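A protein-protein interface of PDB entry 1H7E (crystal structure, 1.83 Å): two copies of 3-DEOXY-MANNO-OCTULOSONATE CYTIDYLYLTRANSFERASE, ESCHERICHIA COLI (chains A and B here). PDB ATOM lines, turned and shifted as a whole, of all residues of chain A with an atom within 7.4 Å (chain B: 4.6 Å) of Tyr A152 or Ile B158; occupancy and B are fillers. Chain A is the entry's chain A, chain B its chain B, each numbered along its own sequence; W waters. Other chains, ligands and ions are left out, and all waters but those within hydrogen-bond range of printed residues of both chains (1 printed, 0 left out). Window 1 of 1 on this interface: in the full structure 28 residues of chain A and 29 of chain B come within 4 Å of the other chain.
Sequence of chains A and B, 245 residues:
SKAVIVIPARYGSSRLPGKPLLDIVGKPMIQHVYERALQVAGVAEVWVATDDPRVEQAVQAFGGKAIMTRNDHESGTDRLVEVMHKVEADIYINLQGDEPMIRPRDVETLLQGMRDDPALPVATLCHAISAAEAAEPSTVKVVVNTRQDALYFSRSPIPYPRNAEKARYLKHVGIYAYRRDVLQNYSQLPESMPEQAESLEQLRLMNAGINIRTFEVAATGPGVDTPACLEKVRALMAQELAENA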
ATOM      1  N   VAL A 140       0.676  18.521 -27.367  1.00  0.00           N
ATOM      2  CA  VAL A 140       1.596  19.441 -26.710  1.00  0.00           C
ATOM      3  C   VAL A 140       2.984  18.810 -26.679  1.00  0.00           C
ATOM      4  O   VAL A 140       3.138  17.667 -26.254  1.00  0.00           O
ATOM      5  CB  VAL A 140       1.099  19.780 -25.254  1.00  0.00           C
ATOM      6  CG1 VAL A 140       2.026  20.780 -24.563  1.00  0.00           C
ATOM      7  CG2 VAL A 140      -0.318  20.326 -25.324  1.00  0.00           C
ATOM      8  N   LYS A 141       3.969  19.533 -27.216  1.00  0.00           N
ATOM      9  CA  LYS A 141       5.349  19.071 -27.243  1.00  0.00           C
ATOM     10  C   LYS A 141       6.105  19.688 -26.071  1.00  0.00           C
ATOM     11  O   LYS A 141       5.744  20.764 -25.569  1.00  0.00           O
ATOM     12  CB  LYS A 141       6.039  19.479 -28.567  1.00  0.00           C
ATOM     13  CG  LYS A 141       5.732  18.568 -29.777  1.00  0.00           C
ATOM     14  CD  LYS A 141       4.294  18.623 -30.266  1.00  0.00           C
ATOM     15  CE  LYS A 141       3.838  20.023 -30.695  1.00  0.00           C
ATOM     16  NZ  LYS A 141       2.537  19.982 -31.455  1.00  0.00           N
ATOM     17  N   VAL A 142       7.132  18.986 -25.616  1.00  0.00           N
ATOM     18  CA  VAL A 142       7.977  19.492 -24.569  1.00  0.00           C
ATOM     19  C   VAL A 142       9.436  19.212 -24.962  1.00  0.00           C
ATOM     20  O   VAL A 142       9.726  18.224 -25.632  1.00  0.00           O
ATOM     21  CB  VAL A 142       7.631  18.858 -23.171  1.00  0.00           C
ATOM     22  CG1 VAL A 142       7.743  17.324 -23.211  1.00  0.00           C
ATOM     23  CG2 VAL A 142       8.535  19.439 -22.077  1.00  0.00           C
ATOM     24  N   VAL A 143      10.333  20.123 -24.594  1.00  0.00           N
ATOM     25  CA  VAL A 143      11.762  19.966 -24.817  1.00  0.00           C
ATOM     26  C   VAL A 143      12.369  20.024 -23.417  1.00  0.00           C
ATOM     27  O   VAL A 143      11.993  20.902 -22.636  1.00  0.00           O
ATOM     28  CB  VAL A 143      12.332  21.109 -25.686  1.00  0.00           C
ATOM     29  CG1 VAL A 143      13.866  21.004 -25.724  1.00  0.00           C
ATOM     30  CG2 VAL A 143      11.781  20.986 -27.097  1.00  0.00           C
ATOM     31  N   VAL A 144      13.312  19.129 -23.116  1.00  0.00           N
ATOM     32  CA  VAL A 144      13.925  19.054 -21.788  1.00  0.00           C
ATOM     33  C   VAL A 144      15.438  19.174 -21.803  1.00  0.00           C
ATOM     34  O   VAL A 144      16.054  18.977 -22.839  1.00  0.00           O
ATOM     35  CB  VAL A 144      13.548  17.699 -21.076  1.00  0.00           C
ATOM     36  CG1 VAL A 144      12.014  17.500 -21.031  1.00  0.00           C
ATOM     37  CG2 VAL A 144      14.204  16.525 -21.791  1.00  0.00           C
ATOM     38  N   ASP A 149      14.497  18.448 -16.847  1.00  0.00           N
ATOM     39  CA  ASP A 149      13.646  19.586 -16.524  1.00  0.00           C
ATOM     40  C   ASP A 149      13.104  20.140 -17.834  1.00  0.00           C
ATOM     41  O   ASP A 149      13.831  20.210 -18.829  1.00  0.00           O
ATOM     42  CB  ASP A 149      14.457  20.687 -15.849  1.00  0.00           C
ATOM     43  CG  ASP A 149      14.956  20.287 -14.471  1.00  0.00           C
ATOM     44  OD1 ASP A 149      14.332  19.417 -13.820  1.00  0.00           O
ATOM     45  OD2 ASP A 149      15.959  20.879 -14.037  1.00  0.00           O
ATOM     46  N   ALA A 150      11.850  20.571 -17.837  1.00  0.00           N
ATOM     47  CA  ALA A 150      11.270  21.137 -19.044  1.00  0.00           C
ATOM     48  C   ALA A 150      11.816  22.532 -19.320  1.00  0.00           C
ATOM     49  O   ALA A 150      12.030  23.333 -18.391  1.00  0.00           O
ATOM     50  CB  ALA A 150       9.748  21.189 -18.934  1.00  0.00           C
ATOM     51  N   LEU A 151      12.127  22.789 -20.594  1.00  0.00           N
ATOM     52  CA  LEU A 151      12.594  24.118 -21.018  1.00  0.00           C
ATOM     53  C   LEU A 151      11.350  24.911 -21.465  1.00  0.00           C
ATOM     54  O   LEU A 151      11.189  26.077 -21.129  1.00  0.00           O
ATOM     55  CB  LEU A 151      13.591  24.012 -22.195  1.00  0.00           C
ATOM     56  CG  LEU A 151      14.932  23.348 -21.865  1.00  0.00           C
ATOM     57  CD1 LEU A 151      15.819  23.358 -23.117  1.00  0.00           C
ATOM     58  CD2 LEU A 151      15.608  24.078 -20.712  1.00  0.00           C
ATOM     59  N   TYR A 152      10.461  24.253 -22.191  1.00  0.00           N
ATOM     60  CA  TYR A 152       9.242  24.908 -22.679  1.00  0.00           C
ATOM     61  C   TYR A 152       8.259  23.840 -23.165  1.00  0.00           C
ATOM     62  O   TYR A 152       8.664  22.710 -23.474  1.00  0.00           O
ATOM     63  CB  TYR A 152       9.599  25.895 -23.831  1.00  0.00           C
ATOM     64  CG  TYR A 152       8.466  26.795 -24.322  1.00  0.00           C
ATOM     65  CD1 TYR A 152       7.842  27.694 -23.460  1.00  0.00           C
ATOM     66  CD2 TYR A 152       8.007  26.726 -25.639  1.00  0.00           C
ATOM     67  CE1 TYR A 152       6.790  28.491 -23.888  1.00  0.00           C
ATOM     68  CE2 TYR A 152       6.946  27.537 -26.078  1.00  0.00           C
ATOM     69  CZ  TYR A 152       6.347  28.409 -25.187  1.00  0.00           C
ATOM     70  OH  TYR A 152       5.294  29.191 -25.577  1.00  0.00           O
ATOM     71  N   PHE A 153       6.968  24.191 -23.186  1.00  0.00           N
ATOM     72  CA  PHE A 153       5.881  23.321 -23.670  1.00  0.00           C
ATOM     73  C   PHE A 153       5.230  24.161 -24.780  1.00  0.00           C
ATOM     74  O   PHE A 153       4.995  25.350 -24.583  1.00  0.00           O
ATOM     75  CB  PHE A 153       4.781  23.100 -22.609  1.00  0.00           C
ATOM     76  CG  PHE A 153       5.205  22.281 -21.422  1.00  0.00           C
ATOM     77  CD1 PHE A 153       5.856  22.881 -20.336  1.00  0.00           C
ATOM     78  CD2 PHE A 153       4.940  20.916 -21.387  1.00  0.00           C
ATOM     79  CE1 PHE A 153       6.253  22.131 -19.211  1.00  0.00           C
ATOM     80  CE2 PHE A 153       5.325  20.142 -20.273  1.00  0.00           C
ATOM     81  CZ  PHE A 153       5.985  20.754 -19.186  1.00  0.00           C
ATOM     82  N   SER A 154       4.880  23.547 -25.903  1.00  0.00           N
ATOM     83  CA  SER A 154       4.262  24.302 -26.980  1.00  0.00           C
ATOM     84  C   SER A 154       3.413  23.461 -27.903  1.00  0.00           C
ATOM     85  O   SER A 154       3.603  22.255 -27.991  1.00  0.00           O
ATOM     86  CB  SER A 154       5.349  24.985 -27.825  1.00  0.00           C
ATOM     87  OG  SER A 154       4.774  25.905 -28.750  1.00  0.00           O
ATOM     88  N   ARG A 155       2.469  24.114 -28.584  1.00  0.00           N
ATOM     89  CA  ARG A 155       1.631  23.463 -29.587  1.00  0.00           C
ATOM     90  C   ARG A 155       2.434  23.492 -30.896  1.00  0.00           C
ATOM     91  O   ARG A 155       2.117  22.759 -31.819  1.00  0.00           O
ATOM     92  CB  ARG A 155       0.300  24.196 -29.762  1.00  0.00           C
ATOM     93  CG  ARG A 155      -0.631  24.013 -28.544  1.00  0.00           C
ATOM     94  CD  ARG A 155      -1.956  24.738 -28.715  1.00  0.00           C
ATOM     95  NE  ARG A 155      -2.709  24.701 -27.464  1.00  0.00           N
ATOM     96  CZ  ARG A 155      -3.312  23.619 -26.975  1.00  0.00           C
ATOM     97  NH1 ARG A 155      -3.282  22.464 -27.632  1.00  0.00           N
ATOM     98  NH2 ARG A 155      -3.870  23.668 -25.778  1.00  0.00           N
ATOM     99  N   SER A 156       3.462  24.343 -30.963  1.00  0.00           N
ATOM    100  CA  SER A 156       4.336  24.395 -32.155  1.00  0.00           C
ATOM    101  C   SER A 156       5.310  23.230 -32.101  1.00  0.00           C
ATOM    102  O   SER A 156       5.716  22.790 -31.020  1.00  0.00           O
ATOM    103  CB  SER A 156       5.213  25.648 -32.200  1.00  0.00           C
ATOM    104  OG  SER A 156       4.493  26.818 -32.487  1.00  0.00           O
ATOM    105  N   PRO A 157       5.714  22.717 -33.273  1.00  0.00           N
ATOM    106  CA  PRO A 157       6.661  21.609 -33.223  1.00  0.00           C
ATOM    107  C   PRO A 157       8.018  22.127 -32.730  1.00  0.00           C
ATOM    108  O   PRO A 157       8.635  22.988 -33.359  1.00  0.00           O
ATOM    109  CB  PRO A 157       6.746  21.153 -34.689  1.00  0.00           C
ATOM    110  CG  PRO A 157       5.450  21.600 -35.275  1.00  0.00           C
ATOM    111  CD  PRO A 157       5.254  22.963 -34.651  1.00  0.00           C
ATOM    112  N   ILE A 158       8.433  21.671 -31.551  1.00  0.00           N
ATOM    113  CA  ILE A 158       9.739  22.037 -31.009  1.00  0.00           C
ATOM    114  C   ILE A 158      10.402  20.698 -30.619  1.00  0.00           C
ATOM    115  O   ILE A 158       9.750  19.830 -30.054  1.00  0.00           O
ATOM    116  CB  ILE A 158       9.650  23.015 -29.767  1.00  0.00           C
ATOM    117  CG1 ILE A 158       8.707  22.466 -28.693  1.00  0.00           C
ATOM    118  CG2 ILE A 158       9.214  24.426 -30.210  1.00  0.00           C
ATOM    119  CD1 ILE A 158       8.793  23.272 -27.383  1.00  0.00           C
ATOM    120  N   MET A 193       1.832  35.734 -20.590  1.00  0.00           N
ATOM    121  CA  MET A 193       1.537  35.910 -21.998  1.00  0.00           C
ATOM    122  C   MET A 193       1.644  34.554 -22.755  1.00  0.00           C
ATOM    123  O   MET A 193       0.754  34.202 -23.514  1.00  0.00           O
ATOM    124  CB  MET A 193       2.444  37.010 -22.585  1.00  0.00           C
ATOM    125  CG  MET A 193       2.267  37.271 -24.092  1.00  0.00           C
ATOM    126  SD  MET A 193       3.121  36.057 -25.116  1.00  0.00           S
ATOM    127  CE  MET A 193       4.742  36.561 -24.783  1.00  0.00           C
ATOM    128  N   PRO A 194       2.724  33.769 -22.547  1.00  0.00           N
ATOM    129  CA  PRO A 194       2.770  32.492 -23.283  1.00  0.00           C
ATOM    130  C   PRO A 194       1.595  31.561 -22.923  1.00  0.00           C
ATOM    131  O   PRO A 194       1.036  30.875 -23.784  1.00  0.00           O
ATOM    132  CB  PRO A 194       4.148  31.923 -22.906  1.00  0.00           C
ATOM    133  CG  PRO A 194       4.972  33.156 -22.748  1.00  0.00           C
ATOM    134  CD  PRO A 194       4.024  34.061 -21.927  1.00  0.00           C
ATOM    135  N   GLU A 195       1.194  31.559 -21.655  1.00  0.00           N
ATOM    136  CA  GLU A 195       0.041  30.754 -21.237  1.00  0.00           C
ATOM    137  C   GLU A 195      -1.226  31.159 -22.018  1.00  0.00           C
ATOM    138  O   GLU A 195      -1.953  30.313 -22.501  1.00  0.00           O
ATOM    139  CB  GLU A 195      -0.236  30.967 -19.733  1.00  0.00           C
ATOM    140  CG  GLU A 195      -1.569  30.315 -19.300  1.00  0.00           C
ATOM    141  CD  GLU A 195      -2.018  30.689 -17.903  1.00  0.00           C
ATOM    142  OE1 GLU A 195      -1.309  31.444 -17.189  1.00  0.00           O
ATOM    143  OE2 GLU A 195      -3.106  30.198 -17.531  1.00  0.00           O
ATOM    144  N   ALA A 197      -1.484  32.967 -24.878  1.00  0.00           N
ATOM    145  CA  ALA A 197      -1.306  32.764 -26.313  1.00  0.00           C
ATOM    146  C   ALA A 197      -1.484  31.288 -26.705  1.00  0.00           C
ATOM    147  O   ALA A 197      -2.231  30.964 -27.621  1.00  0.00           O
ATOM    148  CB  ALA A 197       0.108  33.301 -26.727  1.00  0.00           C
ATOM    149  N   GLU A 198      -0.832  30.383 -25.976  1.00  0.00           N
ATOM    150  CA  GLU A 198      -0.883  28.943 -26.275  1.00  0.00           C
ATOM    151  C   GLU A 198      -2.084  28.218 -25.691  1.00  0.00           C
ATOM    152  O   GLU A 198      -2.448  27.128 -26.151  1.00  0.00           O
ATOM    153  CB  GLU A 198       0.374  28.258 -25.723  1.00  0.00           C
ATOM    154  CG  GLU A 198       1.716  28.763 -26.278  1.00  0.00           C
ATOM    155  CD  GLU A 198       2.450  27.700 -27.067  1.00  0.00           C
ATOM    156  OE1 GLU A 198       1.845  26.651 -27.366  1.00  0.00           O
ATOM    157  OE2 GLU A 198       3.625  27.920 -27.397  1.00  0.00           O
ATOM    158  N   LEU A 200      -2.149  27.066 -22.496  1.00  0.00           N
ATOM    159  CA  LEU A 200      -1.486  25.950 -21.779  1.00  0.00           C
ATOM    160  C   LEU A 200      -1.240  26.438 -20.359  1.00  0.00           C
ATOM    161  O   LEU A 200      -0.340  27.251 -20.094  1.00  0.00           O
ATOM    162  CB  LEU A 200      -0.145  25.546 -22.425  1.00  0.00           C
ATOM    163  CG  LEU A 200      -0.193  24.865 -23.799  1.00  0.00           C
ATOM    164  CD1 LEU A 200       1.237  24.685 -24.375  1.00  0.00           C
ATOM    165  CD2 LEU A 200      -0.943  23.534 -23.683  1.00  0.00           C
ATOM    166  N   GLN A 202       0.068  25.073 -17.747  1.00  0.00           N
ATOM    167  CA  GLN A 202       1.361  24.787 -17.128  1.00  0.00           C
ATOM    168  C   GLN A 202       2.417  25.890 -17.345  1.00  0.00           C
ATOM    169  O   GLN A 202       3.372  26.001 -16.581  1.00  0.00           O
ATOM    170  CB  GLN A 202       1.897  23.409 -17.555  1.00  0.00           C
ATOM    171  CG  GLN A 202       2.215  23.239 -19.058  1.00  0.00           C
ATOM    172  CD  GLN A 202       1.025  22.779 -19.868  1.00  0.00           C
ATOM    173  OE1 GLN A 202      -0.070  23.299 -19.732  1.00  0.00           O
ATOM    174  NE2 GLN A 202       1.242  21.798 -20.737  1.00  0.00           N
ATOM    175  N   LEU A 203       2.226  26.727 -18.364  1.00  0.00           N
ATOM    176  CA  LEU A 203       3.172  27.801 -18.624  1.00  0.00           C
ATOM    177  C   LEU A 203       3.070  28.859 -17.548  1.00  0.00           C
ATOM    178  O   LEU A 203       3.985  29.660 -17.404  1.00  0.00           O
ATOM    179  CB  LEU A 203       2.975  28.401 -20.029  1.00  0.00           C
ATOM    180  CG  LEU A 203       3.315  27.429 -21.174  1.00  0.00           C
ATOM    181  CD1 LEU A 203       3.051  28.077 -22.553  1.00  0.00           C
ATOM    182  CD2 LEU A 203       4.779  26.983 -21.044  1.00  0.00           C
ATOM    183  N   MET A 206       5.927  28.045 -15.231  1.00  0.00           N
ATOM    184  CA  MET A 206       7.215  28.361 -15.818  1.00  0.00           C
ATOM    185  C   MET A 206       7.493  29.850 -15.814  1.00  0.00           C
ATOM    186  O   MET A 206       8.634  30.270 -15.618  1.00  0.00           O
ATOM    187  CB  MET A 206       7.299  27.774 -17.218  1.00  0.00           C
ATOM    188  CG  MET A 206       7.169  26.274 -17.185  1.00  0.00           C
ATOM    189  SD  MET A 206       7.597  25.595 -18.758  1.00  0.00           S
ATOM    190  CE  MET A 206       9.390  25.479 -18.524  1.00  0.00           C
ATOM    191  N   THR A 214      10.117  16.522 -16.170  1.00  0.00           N
ATOM    192  CA  THR A 214       9.279  15.717 -17.052  1.00  0.00           C
ATOM    193  C   THR A 214       9.893  14.361 -17.340  1.00  0.00           C
ATOM    194  O   THR A 214      10.811  14.284 -18.161  1.00  0.00           O
ATOM    195  CB  THR A 214       9.039  16.498 -18.408  1.00  0.00           C
ATOM    196  OG1 THR A 214       8.611  17.832 -18.120  1.00  0.00           O
ATOM    197  CG2 THR A 214       7.943  15.868 -19.229  1.00  0.00           C
ATOM    198  N   LYS B 141      13.364  33.056 -32.470  1.00  0.00           N
ATOM    199  CA  LYS B 141      12.446  33.560 -31.448  1.00  0.00           C
ATOM    200  C   LYS B 141      12.860  33.087 -30.045  1.00  0.00           C
ATOM    201  O   LYS B 141      13.465  32.022 -29.880  1.00  0.00           O
ATOM    202  CB  LYS B 141      11.007  33.097 -31.745  1.00  0.00           C
ATOM    203  CG  LYS B 141      10.266  33.893 -32.834  1.00  0.00           C
ATOM    204  CD  LYS B 141      10.866  33.684 -34.235  1.00  0.00           C
ATOM    205  CE  LYS B 141      10.778  32.236 -34.700  1.00  0.00           C
ATOM    206  NZ  LYS B 141      11.082  32.079 -36.164  1.00  0.00           N
ATOM    207  N   VAL B 143      11.390  33.048 -25.822  1.00  0.00           N
ATOM    208  CA  VAL B 143      10.260  33.234 -24.900  1.00  0.00           C
ATOM    209  C   VAL B 143      10.940  33.347 -23.540  1.00  0.00           C
ATOM    210  O   VAL B 143      11.852  32.577 -23.236  1.00  0.00           O
ATOM    211  CB  VAL B 143       9.246  32.046 -24.923  1.00  0.00           C
ATOM    212  CG1 VAL B 143       8.205  32.253 -23.835  1.00  0.00           C
ATOM    213  CG2 VAL B 143       8.525  32.002 -26.269  1.00  0.00           C
ATOM    214  N   LEU B 151      13.329  30.901 -21.634  1.00  0.00           N
ATOM    215  CA  LEU B 151      12.786  29.562 -21.430  1.00  0.00           C
ATOM    216  C   LEU B 151      13.275  28.664 -22.592  1.00  0.00           C
ATOM    217  O   LEU B 151      13.673  27.511 -22.383  1.00  0.00           O
ATOM    218  CB  LEU B 151      11.255  29.595 -21.409  1.00  0.00           C
ATOM    219  CG  LEU B 151      10.626  30.323 -20.214  1.00  0.00           C
ATOM    220  CD1 LEU B 151       9.118  30.283 -20.349  1.00  0.00           C
ATOM    221  CD2 LEU B 151      11.098  29.667 -18.920  1.00  0.00           C
ATOM    222  N   TYR B 152      13.265  29.204 -23.805  1.00  0.00           N
ATOM    223  CA  TYR B 152      13.706  28.441 -24.970  1.00  0.00           C
ATOM    224  C   TYR B 152      13.922  29.393 -26.142  1.00  0.00           C
ATOM    225  O   TYR B 152      13.349  30.488 -26.164  1.00  0.00           O
ATOM    226  CB  TYR B 152      12.631  27.389 -25.336  1.00  0.00           C
ATOM    227  CG  TYR B 152      13.030  26.345 -26.380  1.00  0.00           C
ATOM    228  CD1 TYR B 152      14.171  25.546 -26.208  1.00  0.00           C
ATOM    229  CD2 TYR B 152      12.293  26.197 -27.569  1.00  0.00           C
ATOM    230  CE1 TYR B 152      14.573  24.636 -27.197  1.00  0.00           C
ATOM    231  CE2 TYR B 152      12.692  25.289 -28.560  1.00  0.00           C
ATOM    232  CZ  TYR B 152      13.843  24.520 -28.362  1.00  0.00           C
ATOM    233  OH  TYR B 152      14.283  23.680 -29.347  1.00  0.00           O
ATOM    234  N   PHE B 153      14.794  28.980 -27.071  1.00  0.00           N
ATOM    235  CA  PHE B 153      15.087  29.715 -28.319  1.00  0.00           C
ATOM    236  C   PHE B 153      14.681  28.755 -29.447  1.00  0.00           C
ATOM    237  O   PHE B 153      15.027  27.568 -29.403  1.00  0.00           O
ATOM    238  CB  PHE B 153      16.596  29.999 -28.471  1.00  0.00           C
ATOM    239  CG  PHE B 153      17.149  30.969 -27.479  1.00  0.00           C
ATOM    240  CD1 PHE B 153      17.588  30.530 -26.218  1.00  0.00           C
ATOM    241  CD2 PHE B 153      17.284  32.319 -27.809  1.00  0.00           C
ATOM    242  CE1 PHE B 153      18.155  31.421 -25.299  1.00  0.00           C
ATOM    243  CE2 PHE B 153      17.855  33.225 -26.893  1.00  0.00           C
ATOM    244  CZ  PHE B 153      18.290  32.764 -25.631  1.00  0.00           C
ATOM    245  N   SER B 154      13.958  29.243 -30.452  1.00  0.00           N
ATOM    246  CA  SER B 154      13.548  28.372 -31.540  1.00  0.00           C
ATOM    247  C   SER B 154      13.324  29.095 -32.864  1.00  0.00           C
ATOM    248  O   SER B 154      13.075  30.300 -32.901  1.00  0.00           O
ATOM    249  CB  SER B 154      12.239  27.652 -31.161  1.00  0.00           C
ATOM    250  OG  SER B 154      11.903  26.618 -32.075  1.00  0.00           O
ATOM    251  N   SER B 156      10.932  27.844 -34.668  1.00  0.00           N
ATOM    252  CA  SER B 156       9.479  27.685 -34.746  1.00  0.00           C
ATOM    253  C   SER B 156       8.862  28.928 -34.111  1.00  0.00           C
ATOM    254  O   SER B 156       9.469  29.564 -33.245  1.00  0.00           O
ATOM    255  CB  SER B 156       9.000  26.487 -33.928  1.00  0.00           C
ATOM    256  OG  SER B 156       9.096  25.283 -34.650  1.00  0.00           O
ATOM    257  N   PRO B 157       7.659  29.316 -34.564  1.00  0.00           N
ATOM    258  CA  PRO B 157       7.020  30.491 -33.983  1.00  0.00           C
ATOM    259  C   PRO B 157       6.533  30.143 -32.565  1.00  0.00           C
ATOM    260  O   PRO B 157       5.640  29.310 -32.397  1.00  0.00           O
ATOM    261  CB  PRO B 157       5.812  30.727 -34.901  1.00  0.00           C
ATOM    262  CG  PRO B 157       6.139  29.978 -36.163  1.00  0.00           C
ATOM    263  CD  PRO B 157       6.853  28.764 -35.664  1.00  0.00           C
ATOM    264  N   ILE B 158       7.190  30.700 -31.560  1.00  0.00           N
ATOM    265  CA  ILE B 158       6.798  30.490 -30.162  1.00  0.00           C
ATOM    266  C   ILE B 158       6.664  31.878 -29.549  1.00  0.00           C
ATOM    267  O   ILE B 158       7.487  32.762 -29.809  1.00  0.00           O
ATOM    268  CB  ILE B 158       7.832  29.629 -29.346  1.00  0.00           C
ATOM    269  CG1 ILE B 158       9.243  30.205 -29.457  1.00  0.00           C
ATOM    270  CG2 ILE B 158       7.801  28.192 -29.828  1.00  0.00           C
ATOM    271  CD1 ILE B 158      10.257  29.508 -28.554  1.00  0.00           C
ATOM    272  N   PRO B 159       5.589  32.109 -28.773  1.00  0.00           N
ATOM    273  CA  PRO B 159       4.540  31.127 -28.475  1.00  0.00           C
ATOM    274  C   PRO B 159       3.602  30.867 -29.642  1.00  0.00           C
ATOM    275  O   PRO B 159       3.377  31.755 -30.473  1.00  0.00           O
ATOM    276  CB  PRO B 159       3.786  31.777 -27.317  1.00  0.00           C
ATOM    277  CG  PRO B 159       3.918  33.239 -27.627  1.00  0.00           C
ATOM    278  CD  PRO B 159       5.349  33.377 -28.066  1.00  0.00           C
ATOM    279  N   TYR B 160       3.076  29.640 -29.698  1.00  0.00           N
ATOM    280  CA  TYR B 160       2.117  29.245 -30.716  1.00  0.00           C
ATOM    281  C   TYR B 160       0.904  30.163 -30.543  1.00  0.00           C
ATOM    282  O   TYR B 160       0.398  30.321 -29.428  1.00  0.00           O
ATOM    283  CB  TYR B 160       1.700  27.792 -30.521  1.00  0.00           C
ATOM    284  CG  TYR B 160       0.694  27.329 -31.546  1.00  0.00           C
ATOM    285  CD1 TYR B 160       1.111  26.830 -32.777  1.00  0.00           C
ATOM    286  CD2 TYR B 160      -0.663  27.419 -31.298  1.00  0.00           C
ATOM    287  CE1 TYR B 160       0.197  26.431 -33.739  1.00  0.00           C
ATOM    288  CE2 TYR B 160      -1.592  27.024 -32.245  1.00  0.00           C
ATOM    289  CZ  TYR B 160      -1.155  26.529 -33.469  1.00  0.00           C
ATOM    290  OH  TYR B 160      -2.077  26.117 -34.411  1.00  0.00           O
ATOM    291  N   TYR B 169       5.769  38.496 -29.880  1.00  0.00           N
ATOM    292  CA  TYR B 169       7.001  37.827 -30.315  1.00  0.00           C
ATOM    293  C   TYR B 169       8.290  38.602 -30.105  1.00  0.00           C
ATOM    294  O   TYR B 169       8.301  39.820 -30.183  1.00  0.00           O
ATOM    295  CB  TYR B 169       6.876  37.403 -31.779  1.00  0.00           C
ATOM    296  CG  TYR B 169       5.799  36.379 -31.998  1.00  0.00           C
ATOM    297  CD1 TYR B 169       6.052  35.023 -31.774  1.00  0.00           C
ATOM    298  CD2 TYR B 169       4.511  36.763 -32.377  1.00  0.00           C
ATOM    299  CE1 TYR B 169       5.047  34.076 -31.912  1.00  0.00           C
ATOM    300  CE2 TYR B 169       3.488  35.820 -32.521  1.00  0.00           C
ATOM    301  CZ  TYR B 169       3.772  34.484 -32.280  1.00  0.00           C
ATOM    302  OH  TYR B 169       2.772  33.554 -32.387  1.00  0.00           O
HETATM  303  O   HOH W   1      12.796  26.776 -19.075  1.00  0.00           O
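Hydrophobic or aromatic side chains of chain A that line the printed part of chain B: Val A143, Leu A151, Tyr A152, Ile A158, Met A193, Pro A194 and Ala A197. Hydrophobic or aromatic side chains of chain B within 4 Å of the printed part of chain A: Val B143, Leu B151, Tyr B152, Ile B158, Pro B159 and Tyr B160. Along chain B the printed residues that touch a printed residue of chain A span positions 143 to 160. Among the printed residues, no Asp or Glu carboxylate lies within 4 Å of a Lys or Arg side-chain nitrogen of the other chain.
The backbone NH (N) of Lys A141 lies within hydrogen-bond range of the backbone carbonyl oxygen (O) of Ser A154 (2.9 Å). OH of Tyr A152 is in hydrogen-bond range of OE2 of Glu A198, 2.8 Å away. The side-chain hydroxyl (OG) of Ser A154 lies within hydrogen-bond range of the backbone NH (N) of Ser A156. OG of Ser A154 lies within hydrogen-bond range of OE2 of Glu A198, 2.7 Å away. O of Val B143 sits at hydrogen-bond distance from N of Leu B151 (2.7 Å). O of Tyr B152 is in hydrogen-bond range of N of Val B143 (3.2 Å).
Val A143 touches Tyr B152, but with the chains exchanged Tyr A152 does not touch Val B143 (4.02 Å). Tyr A152 touches Ile B158, and with the chains exchanged Ile A158 touches Tyr B152. Ser A154 touches Ile B158, and with the chains exchanged Ile A158 touches Ser B154. Ser A156 touches Pro B157, and with the chains exchanged Pro A157 touches Ser B156. 9 positions are printed for both chains.
Of chain A, only Tyr A152 (3.9 Å) and Ser A154 (3.9 Å) come within 4 Å of Ile B158. Printed residues of chain B within 4 Å of Pro A194: Val B143 (3.5 Å). Of the printed residues of chain A, Val B143 touches Pro A194 (3.5 Å). Of the printed residues of chain B, Ile A158 touches Tyr B152 (3.9 Å) and Ser B154 (3.9 Å). Printed residues of chain B within 4 Å of Leu A151: Leu B151. Of the printed residues of chain B, Pro A157 touches Ser B156 (2.7 Å). The nearest printed residue of chain A that does not touch Leu B151 is Met A206 (4.2 Å).
The side-chain hydroxyl (OG) of Ser A156 is in hydrogen-bond range of the backbone carbonyl oxygen (O) of Pro B157 (2.7 Å). The side-chain hydroxyl of Ser B156 is in hydrogen-bond range of the backbone carbonyl oxygen of Pro A157. OE2 of Glu A198 is in hydrogen-bond range of N of Tyr B160 (2.9 Å). The backbone carbonyl oxygen (O) of Leu A151 lies close to the backbone carbonyl oxygen (O) of Leu B151 (3.1 Å). The backbone carbonyl oxygen of Tyr B160 sits close to the backbone carbonyl oxygen of Ala A197.
Val A143 touches Tyr B152 (CG1 to CE1, 3.98 Å). Tyr B152 touches Tyr A152. Tyr A152 touches Ile B158 (CE2 to CG2, 3.9 Å). OH of Tyr A152 touches CB of Pro B159, at 3.5 Å. Arg A155 touches Tyr B160. CG2 of Ile A158 touches CE2 of Tyr B152, at 3.9 Å. Ile A158 touches Ser B154 (CG2 to OG, 3.9 Å). Met A193 touches Pro B159. CG1 of Val B143 touches CG of Pro A194, at 3.5 Å. Glu A198 touches Pro B159.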
